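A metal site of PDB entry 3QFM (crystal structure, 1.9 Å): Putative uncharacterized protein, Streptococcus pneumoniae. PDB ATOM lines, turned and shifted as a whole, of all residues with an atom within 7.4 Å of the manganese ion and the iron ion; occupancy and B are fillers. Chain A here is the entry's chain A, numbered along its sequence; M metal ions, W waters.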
ATOM      1  N   SER A  18     -23.413 -21.043  -9.172  1.00  0.00           N
ATOM      2  CA  SER A  18     -23.134 -22.219 -10.000  1.00  0.00           C
ATOM      3  C   SER A  18     -22.910 -21.860 -11.483  1.00  0.00           C
ATOM      4  O   SER A  18     -23.544 -20.917 -12.001  1.00  0.00           O
ATOM      5  CB  SER A  18     -24.323 -23.194  -9.921  1.00  0.00           C
ATOM      6  OG  SER A  18     -23.904 -24.488 -10.362  1.00  0.00           O
ATOM      7  N   ASP A  19     -22.053 -22.618 -12.155  1.00  0.00           N
ATOM      8  CA  ASP A  19     -21.974 -22.566 -13.621  1.00  0.00           C
ATOM      9  C   ASP A  19     -21.745 -21.125 -14.094  1.00  0.00           C
ATOM     10  O   ASP A  19     -22.492 -20.554 -14.933  1.00  0.00           O
ATOM     11  CB  ASP A  19     -23.270 -23.188 -14.216  1.00  0.00           C
ATOM     12  CG  ASP A  19     -23.418 -24.659 -13.830  1.00  0.00           C
ATOM     13  OD1 ASP A  19     -24.214 -24.986 -12.947  1.00  0.00           O
ATOM     14  OD2 ASP A  19     -22.685 -25.505 -14.373  1.00  0.00           O
ATOM     15  N   ILE A  20     -20.717 -20.522 -13.511  1.00  0.00           N
ATOM     16  CA  ILE A  20     -20.248 -19.192 -13.896  1.00  0.00           C
ATOM     17  C   ILE A  20     -19.676 -19.212 -15.318  1.00  0.00           C
ATOM     18  O   ILE A  20     -19.899 -18.279 -16.106  1.00  0.00           O
ATOM     19  CB  ILE A  20     -19.165 -18.696 -12.870  1.00  0.00           C
ATOM     20  CG1 ILE A  20     -19.780 -18.661 -11.476  1.00  0.00           C
ATOM     21  CG2 ILE A  20     -18.574 -17.344 -13.255  1.00  0.00           C
ATOM     22  CD1 ILE A  20     -18.725 -18.620 -10.335  1.00  0.00           C
ATOM     23  N   HIS A  21     -18.945 -20.265 -15.632  1.00  0.00           N
ATOM     24  CA  HIS A  21     -18.454 -20.512 -16.982  1.00  0.00           C
ATOM     25  C   HIS A  21     -17.671 -19.310 -17.551  1.00  0.00           C
ATOM     26  O   HIS A  21     -17.764 -18.958 -18.739  1.00  0.00           O
ATOM     27  CB  HIS A  21     -19.605 -20.953 -17.890  1.00  0.00           C
ATOM     28  CG  HIS A  21     -19.945 -22.398 -17.741  1.00  0.00           C
ATOM     29  ND1 HIS A  21     -19.099 -23.408 -18.144  1.00  0.00           N
ATOM     30  CD2 HIS A  21     -21.011 -23.015 -17.147  1.00  0.00           C
ATOM     31  CE1 HIS A  21     -19.627 -24.580 -17.841  1.00  0.00           C
ATOM     32  NE2 HIS A  21     -20.790 -24.361 -17.246  1.00  0.00           N
ATOM     33  N   LEU A  45     -20.785 -24.249  -6.588  1.00  0.00           N
ATOM     34  CA  LEU A  45     -21.202 -25.548  -7.112  1.00  0.00           C
ATOM     35  C   LEU A  45     -20.388 -26.031  -8.305  1.00  0.00           C
ATOM     36  O   LEU A  45     -20.677 -27.100  -8.840  1.00  0.00           O
ATOM     37  CB  LEU A  45     -22.715 -25.565  -7.467  1.00  0.00           C
ATOM     38  CG  LEU A  45     -23.730 -25.164  -6.383  1.00  0.00           C
ATOM     39  CD1 LEU A  45     -25.115 -25.759  -6.689  1.00  0.00           C
ATOM     40  CD2 LEU A  45     -23.306 -25.536  -4.944  1.00  0.00           C
ATOM     41  N   GLY A  46     -19.353 -25.270  -8.698  1.00  0.00           N
ATOM     42  CA  GLY A  46     -18.496 -25.687  -9.803  1.00  0.00           C
ATOM     43  C   GLY A  46     -18.798 -25.129 -11.204  1.00  0.00           C
ATOM     44  O   GLY A  46     -19.790 -24.388 -11.414  1.00  0.00           O
ATOM     45  N   ASP A  47     -17.930 -25.485 -12.149  1.00  0.00           N
ATOM     46  CA  ASP A  47     -17.962 -24.945 -13.532  1.00  0.00           C
ATOM     47  C   ASP A  47     -17.662 -23.453 -13.509  1.00  0.00           C
ATOM     48  O   ASP A  47     -18.495 -22.587 -13.854  1.00  0.00           O
ATOM     49  CB  ASP A  47     -19.276 -25.290 -14.259  1.00  0.00           C
ATOM     50  CG  ASP A  47     -19.303 -26.699 -14.766  1.00  0.00           C
ATOM     51  OD1 ASP A  47     -18.360 -27.461 -14.430  1.00  0.00           O
ATOM     52  OD2 ASP A  47     -20.267 -27.054 -15.487  1.00  0.00           O
ATOM     53  N   ILE A  48     -16.441 -23.155 -13.053  1.00  0.00           N
ATOM     54  CA  ILE A  48     -16.037 -21.796 -12.760  1.00  0.00           C
ATOM     55  C   ILE A  48     -15.527 -21.027 -13.987  1.00  0.00           C
ATOM     56  O   ILE A  48     -15.997 -19.924 -14.282  1.00  0.00           O
ATOM     57  CB  ILE A  48     -14.968 -21.814 -11.638  1.00  0.00           C
ATOM     58  CG1 ILE A  48     -15.563 -22.499 -10.389  1.00  0.00           C
ATOM     59  CG2 ILE A  48     -14.478 -20.399 -11.332  1.00  0.00           C
ATOM     60  CD1 ILE A  48     -14.447 -22.892  -9.373  1.00  0.00           C
ATOM     61  N   MET A  50     -14.374 -20.961 -18.251  1.00  0.00           N
ATOM     62  CA  MET A  50     -14.603 -21.422 -19.634  1.00  0.00           C
ATOM     63  C   MET A  50     -16.084 -21.688 -19.879  1.00  0.00           C
ATOM     64  O   MET A  50     -16.753 -22.202 -18.998  1.00  0.00           O
ATOM     65  CB  MET A  50     -13.797 -22.680 -19.969  1.00  0.00           C
ATOM     66  CG  MET A  50     -12.296 -22.548 -19.692  1.00  0.00           C
ATOM     67  SD  MET A  50     -11.421 -24.039 -20.175  1.00  0.00           S
ATOM     68  CE  MET A  50     -12.202 -25.302 -19.186  1.00  0.00           C
ATOM     69  N   LEU A  72     -16.594 -29.902  -6.917  1.00  0.00           N
ATOM     70  CA  LEU A  72     -15.972 -30.044  -8.230  1.00  0.00           C
ATOM     71  C   LEU A  72     -16.955 -30.173  -9.412  1.00  0.00           C
ATOM     72  O   LEU A  72     -17.732 -31.124  -9.465  1.00  0.00           O
ATOM     73  CB  LEU A  72     -15.080 -31.279  -8.232  1.00  0.00           C
ATOM     74  CG  LEU A  72     -14.178 -31.546  -9.438  1.00  0.00           C
ATOM     75  CD1 LEU A  72     -13.001 -30.520  -9.508  1.00  0.00           C
ATOM     76  CD2 LEU A  72     -13.636 -32.954  -9.299  1.00  0.00           C
ATOM     77  N   GLY A  73     -16.810 -29.271 -10.378  1.00  0.00           N
ATOM     78  CA  GLY A  73     -17.591 -29.331 -11.618  1.00  0.00           C
ATOM     79  C   GLY A  73     -16.855 -30.088 -12.705  1.00  0.00           C
ATOM     80  O   GLY A  73     -15.613 -30.169 -12.692  1.00  0.00           O
ATOM     81  N   ASN A  74     -17.595 -30.617 -13.662  1.00  0.00           N
ATOM     82  CA  ASN A  74     -16.924 -31.281 -14.794  1.00  0.00           C
ATOM     83  C   ASN A  74     -15.940 -30.408 -15.599  1.00  0.00           C
ATOM     84  O   ASN A  74     -14.913 -30.920 -16.072  1.00  0.00           O
ATOM     85  CB  ASN A  74     -17.933 -31.997 -15.707  1.00  0.00           C
ATOM     86  CG  ASN A  74     -18.969 -31.067 -16.323  1.00  0.00           C
ATOM     87  OD1 ASN A  74     -19.604 -30.226 -15.621  1.00  0.00           O
ATOM     88  ND2 ASN A  74     -19.181 -31.233 -17.649  1.00  0.00           N
ATOM     89  N   TRP A  75     -16.223 -29.124 -15.729  1.00  0.00           N
ATOM     90  CA  TRP A  75     -15.304 -28.209 -16.448  1.00  0.00           C
ATOM     91  C   TRP A  75     -13.971 -27.954 -15.715  1.00  0.00           C
ATOM     92  O   TRP A  75     -12.989 -27.537 -16.338  1.00  0.00           O
ATOM     93  CB  TRP A  75     -16.000 -26.892 -16.815  1.00  0.00           C
ATOM     94  CG  TRP A  75     -16.979 -27.082 -17.952  1.00  0.00           C
ATOM     95  CD1 TRP A  75     -18.122 -27.852 -17.947  1.00  0.00           C
ATOM     96  CD2 TRP A  75     -16.906 -26.493 -19.254  1.00  0.00           C
ATOM     97  NE1 TRP A  75     -18.751 -27.773 -19.173  1.00  0.00           N
ATOM     98  CE2 TRP A  75     -18.031 -26.941 -19.993  1.00  0.00           C
ATOM     99  CE3 TRP A  75     -16.001 -25.618 -19.871  1.00  0.00           C
ATOM    100  CZ2 TRP A  75     -18.271 -26.549 -21.324  1.00  0.00           C
ATOM    101  CZ3 TRP A  75     -16.233 -25.219 -21.203  1.00  0.00           C
ATOM    102  CH2 TRP A  75     -17.368 -25.697 -21.910  1.00  0.00           C
ATOM    103  N   HIS A 136     -22.031 -31.035  -7.789  1.00  0.00           N
ATOM    104  CA  HIS A 136     -22.243 -30.342  -9.054  1.00  0.00           C
ATOM    105  C   HIS A 136     -23.363 -31.032  -9.850  1.00  0.00           C
ATOM    106  O   HIS A 136     -24.283 -30.403 -10.322  1.00  0.00           O
ATOM    107  CB  HIS A 136     -20.972 -30.355  -9.917  1.00  0.00           C
ATOM    108  CG  HIS A 136     -21.135 -29.598 -11.200  1.00  0.00           C
ATOM    109  ND1 HIS A 136     -21.345 -28.231 -11.226  1.00  0.00           N
ATOM    110  CD2 HIS A 136     -21.119 -30.005 -12.488  1.00  0.00           C
ATOM    111  CE1 HIS A 136     -21.425 -27.828 -12.475  1.00  0.00           C
ATOM    112  NE2 HIS A 136     -21.309 -28.878 -13.265  1.00  0.00           N
ATOM    113  N   HIS A 137     -23.257 -32.335  -9.986  1.00  0.00           N
ATOM    114  CA  HIS A 137     -24.312 -33.088 -10.630  1.00  0.00           C
ATOM    115  C   HIS A 137     -24.695 -34.210  -9.653  1.00  0.00           C
ATOM    116  O   HIS A 137     -25.220 -33.919  -8.570  1.00  0.00           O
ATOM    117  CB  HIS A 137     -23.788 -33.584 -11.995  1.00  0.00           C
ATOM    118  CG  HIS A 137     -24.827 -34.272 -12.824  1.00  0.00           C
ATOM    119  ND1 HIS A 137     -24.526 -35.352 -13.627  1.00  0.00           N
ATOM    120  CD2 HIS A 137     -26.163 -34.060 -12.944  1.00  0.00           C
ATOM    121  CE1 HIS A 137     -25.624 -35.740 -14.252  1.00  0.00           C
ATOM    122  NE2 HIS A 137     -26.635 -34.983 -13.850  1.00  0.00           N
ATOM    123  N   ASN A 142     -19.774 -35.908 -11.880  1.00  0.00           N
ATOM    124  CA  ASN A 142     -20.060 -34.465 -12.128  1.00  0.00           C
ATOM    125  C   ASN A 142     -20.452 -34.084 -13.564  1.00  0.00           C
ATOM    126  O   ASN A 142     -20.544 -32.885 -13.891  1.00  0.00           O
ATOM    127  CB  ASN A 142     -18.942 -33.558 -11.600  1.00  0.00           C
ATOM    128  CG  ASN A 142     -17.597 -33.743 -12.304  1.00  0.00           C
ATOM    129  OD1 ASN A 142     -17.519 -34.361 -13.371  1.00  0.00           O
ATOM    130  ND2 ASN A 142     -16.540 -33.210 -11.715  1.00  0.00           N
ATOM    131  N   TRP A 143     -20.676 -35.096 -14.392  1.00  0.00           N
ATOM    132  CA  TRP A 143     -20.967 -34.897 -15.824  1.00  0.00           C
ATOM    133  C   TRP A 143     -22.110 -35.813 -16.252  1.00  0.00           C
ATOM    134  O   TRP A 143     -22.467 -36.730 -15.521  1.00  0.00           O
ATOM    135  CB  TRP A 143     -19.707 -35.210 -16.674  1.00  0.00           C
ATOM    136  CG  TRP A 143     -19.164 -36.609 -16.430  1.00  0.00           C
ATOM    137  CD1 TRP A 143     -18.339 -36.997 -15.396  1.00  0.00           C
ATOM    138  CD2 TRP A 143     -19.416 -37.786 -17.195  1.00  0.00           C
ATOM    139  NE1 TRP A 143     -18.066 -38.324 -15.477  1.00  0.00           N
ATOM    140  CE2 TRP A 143     -18.703 -38.841 -16.576  1.00  0.00           C
ATOM    141  CE3 TRP A 143     -20.161 -38.058 -18.353  1.00  0.00           C
ATOM    142  CZ2 TRP A 143     -18.709 -40.146 -17.088  1.00  0.00           C
ATOM    143  CZ3 TRP A 143     -20.177 -39.362 -18.852  1.00  0.00           C
ATOM    144  CH2 TRP A 143     -19.459 -40.383 -18.209  1.00  0.00           C
ATOM    145  N   GLY A 144     -22.666 -35.549 -17.426  1.00  0.00           N
ATOM    146  CA  GLY A 144     -23.740 -36.384 -17.969  1.00  0.00           C
ATOM    147  C   GLY A 144     -25.108 -35.734 -17.991  1.00  0.00           C
ATOM    148  O   GLY A 144     -25.257 -34.534 -17.698  1.00  0.00           O
ATOM    149  N   GLY A 171     -26.090 -28.258  -9.491  1.00  0.00           N
ATOM    150  CA  GLY A 171     -26.042 -27.281 -10.599  1.00  0.00           C
ATOM    151  C   GLY A 171     -25.972 -28.069 -11.912  1.00  0.00           C
ATOM    152  O   GLY A 171     -26.807 -28.935 -12.128  1.00  0.00           O
ATOM    153  N   HIS A 172     -24.980 -27.791 -12.762  1.00  0.00           N
ATOM    154  CA  HIS A 172     -24.702 -28.599 -13.988  1.00  0.00           C
ATOM    155  C   HIS A 172     -25.699 -28.439 -15.166  1.00  0.00           C
ATOM    156  O   HIS A 172     -25.300 -28.330 -16.328  1.00  0.00           O
ATOM    157  CB  HIS A 172     -24.517 -30.107 -13.667  1.00  0.00           C
ATOM    158  CG  HIS A 172     -24.094 -30.927 -14.851  1.00  0.00           C
ATOM    159  ND1 HIS A 172     -22.909 -30.692 -15.529  1.00  0.00           N
ATOM    160  CD2 HIS A 172     -24.690 -31.967 -15.486  1.00  0.00           C
ATOM    161  CE1 HIS A 172     -22.798 -31.571 -16.529  1.00  0.00           C
ATOM    162  NE2 HIS A 172     -23.858 -32.363 -16.508  1.00  0.00           N
ATOM    163  N   ILE A 173     -26.994 -28.460 -14.873  1.00  0.00           N
ATOM    164  CA  ILE A 173     -27.987 -28.400 -15.959  1.00  0.00           C
ATOM    165  C   ILE A 173     -28.399 -26.996 -16.415  1.00  0.00           C
ATOM    166  O   ILE A 173     -29.049 -26.875 -17.454  1.00  0.00           O
ATOM    167  CB  ILE A 173     -29.217 -29.295 -15.651  1.00  0.00           C
ATOM    168  CG1 ILE A 173     -30.013 -28.751 -14.456  1.00  0.00           C
ATOM    169  CG2 ILE A 173     -28.736 -30.727 -15.404  1.00  0.00           C
ATOM    170  CD1 ILE A 173     -31.471 -29.305 -14.394  1.00  0.00           C
ATOM    171  N   HIS A 174     -27.972 -25.956 -15.672  1.00  0.00           N
ATOM    172  CA  HIS A 174     -28.213 -24.550 -16.030  1.00  0.00           C
ATOM    173  C   HIS A 174     -29.716 -24.179 -16.066  1.00  0.00           C
ATOM    174  O   HIS A 174     -30.138 -23.321 -16.859  1.00  0.00           O
ATOM    175  CB  HIS A 174     -27.576 -24.183 -17.377  1.00  0.00           C
ATOM    176  CG  HIS A 174     -26.092 -24.402 -17.434  1.00  0.00           C
ATOM    177  ND1 HIS A 174     -25.318 -23.793 -18.386  1.00  0.00           N
ATOM    178  CD2 HIS A 174     -25.251 -25.135 -16.670  1.00  0.00           C
ATOM    179  CE1 HIS A 174     -24.049 -24.134 -18.199  1.00  0.00           C
ATOM    180  NE2 HIS A 174     -23.985 -24.961 -17.168  1.00  0.00           N
ATOM    181  N   SER A 192     -27.751 -21.267 -13.733  1.00  0.00           N
ATOM    182  CA  SER A 192     -26.389 -20.882 -14.163  1.00  0.00           C
ATOM    183  C   SER A 192     -26.212 -19.383 -14.157  1.00  0.00           C
ATOM    184  O   SER A 192     -27.022 -18.637 -14.719  1.00  0.00           O
ATOM    185  CB  SER A 192     -26.105 -21.413 -15.591  1.00  0.00           C
ATOM    186  OG  SER A 192     -24.854 -20.958 -16.055  1.00  0.00           O
ATOM    187  N   GLN A 195     -24.302 -18.993 -18.168  1.00  0.00           N
ATOM    188  CA  GLN A 195     -24.823 -19.689 -19.359  1.00  0.00           C
ATOM    189  C   GLN A 195     -26.245 -20.225 -19.107  1.00  0.00           C
ATOM    190  O   GLN A 195     -26.488 -21.419 -19.240  1.00  0.00           O
ATOM    191  CB  GLN A 195     -23.907 -20.861 -19.768  1.00  0.00           C
ATOM    192  CG  GLN A 195     -22.443 -20.524 -20.053  1.00  0.00           C
ATOM    193  CD  GLN A 195     -22.214 -19.948 -21.453  1.00  0.00           C
ATOM    194  OE1 GLN A 195     -21.731 -20.637 -22.348  1.00  0.00           O
ATOM    195  NE2 GLN A 195     -22.573 -18.676 -21.636  1.00  0.00           N
ATOM    196  N   PHE A 267     -22.208 -29.118 -23.221  1.00  0.00           N
ATOM    197  CA  PHE A 267     -22.417 -29.083 -21.762  1.00  0.00           C
ATOM    198  C   PHE A 267     -22.915 -30.432 -21.215  1.00  0.00           C
ATOM    199  O   PHE A 267     -22.518 -30.859 -20.118  1.00  0.00           O
ATOM    200  CB  PHE A 267     -23.411 -27.982 -21.381  1.00  0.00           C
ATOM    201  CG  PHE A 267     -22.884 -26.562 -21.511  1.00  0.00           C
ATOM    202  CD1 PHE A 267     -23.524 -25.643 -22.342  1.00  0.00           C
ATOM    203  CD2 PHE A 267     -21.777 -26.140 -20.771  1.00  0.00           C
ATOM    204  CE1 PHE A 267     -23.061 -24.335 -22.456  1.00  0.00           C
ATOM    205  CE2 PHE A 267     -21.298 -24.835 -20.879  1.00  0.00           C
ATOM    206  CZ  PHE A 267     -21.941 -23.915 -21.720  1.00  0.00           C
ATOM    207  N   LEU A 268     -23.795 -31.093 -21.970  1.00  0.00           N
ATOM    208  CA  LEU A 268     -24.519 -32.263 -21.498  1.00  0.00           C
ATOM    209  C   LEU A 268     -24.273 -33.495 -22.385  1.00  0.00           C
ATOM    210  O   LEU A 268     -23.390 -34.323 -22.091  1.00  0.00           O
ATOM    211  CB  LEU A 268     -26.032 -31.933 -21.420  1.00  0.00           C
ATOM    212  CG  LEU A 268     -26.467 -30.764 -20.509  1.00  0.00           C
ATOM    213  CD1 LEU A 268     -27.880 -30.254 -20.846  1.00  0.00           C
ATOM    214  CD2 LEU A 268     -26.350 -31.088 -19.022  1.00  0.00           C
HETATM  215 MN    MN M   1     -21.345 -29.044 -15.442  1.00  0.00          MN
HETATM  216 FE    FE M   2     -22.032 -25.893 -16.346  1.00  0.00          FE
HETATM  217  O   HOH W   1     -21.205 -29.104 -18.574  1.00  0.00           O
HETATM  218  O   HOH W   2     -22.458 -27.717 -16.474  1.00  0.00           O
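The nearest printed residue that does not touch the iron ion is His 172 (4.1 Å).
Water W2 binds the iron ion.
The side-chain carboxylate (OD2) of Asp 19 binds the iron ion (2.1 Å).
The iron ion is bound by NE2 of His 21.
OD2 of Asp 47 is bound to the iron ion (2.3 Å).
NE2 of His 174 binds the iron ion (2.3 Å).
The iron ion has five donor atoms within binding distance.
The manganese ion is bound by water W2 (2.0 Å), OD1 of Asn 74 (2.1 Å), NE2 of His 136 (2.2 Å), OD2 of Asp 47 (2.3 Å) and ND1 of His 172 (2.3 Å).
The manganese ion has five donor atoms within binding distance.
Of the 26 residues printed, 5 come within 4 Å of the manganese ion.
The nearest printed residue that does not touch the manganese ion is Asn 142 (4.2 Å).
Water W1 lies within hydrogen-bond range of the backbone carbonyl oxygen of Phe 267 (2.7 Å), the indole nitrogen of Trp 75 (2.9 Å) and the side-chain amide nitrogen of Asn 74 (3.1 Å).
The side-chain carboxylate (OD1) of Asp 19 is in hydrogen-bond range of the side-chain hydroxyl (OG) of Ser 18 (2.7 Å).
A ring nitrogen (ND1) of His 21 lies within hydrogen-bond range of the backbone carbonyl oxygen (O) of Met 50 (2.8 Å).
N of His 21 is in hydrogen-bond range of O of Ile 48, 3.3 Å away.
N of Gly 171 lies within hydrogen-bond range of O of His 136, 2.9 Å away.
The backbone carbonyl oxygen of Leu 45 lies within hydrogen-bond range of a ring nitrogen (ND1) of His 136, at 2.7 Å.
The side-chain carboxylate (OD1) of Asp 47 lies within hydrogen-bond range of the backbone NH (N) of Trp 75.
O of Gly 144 sits at hydrogen-bond distance from NE2 of His 172, at 2.8 Å.
A ring nitrogen (ND1) of His 174 is in hydrogen-bond range of the backbone carbonyl oxygen (O) of Gln 195.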
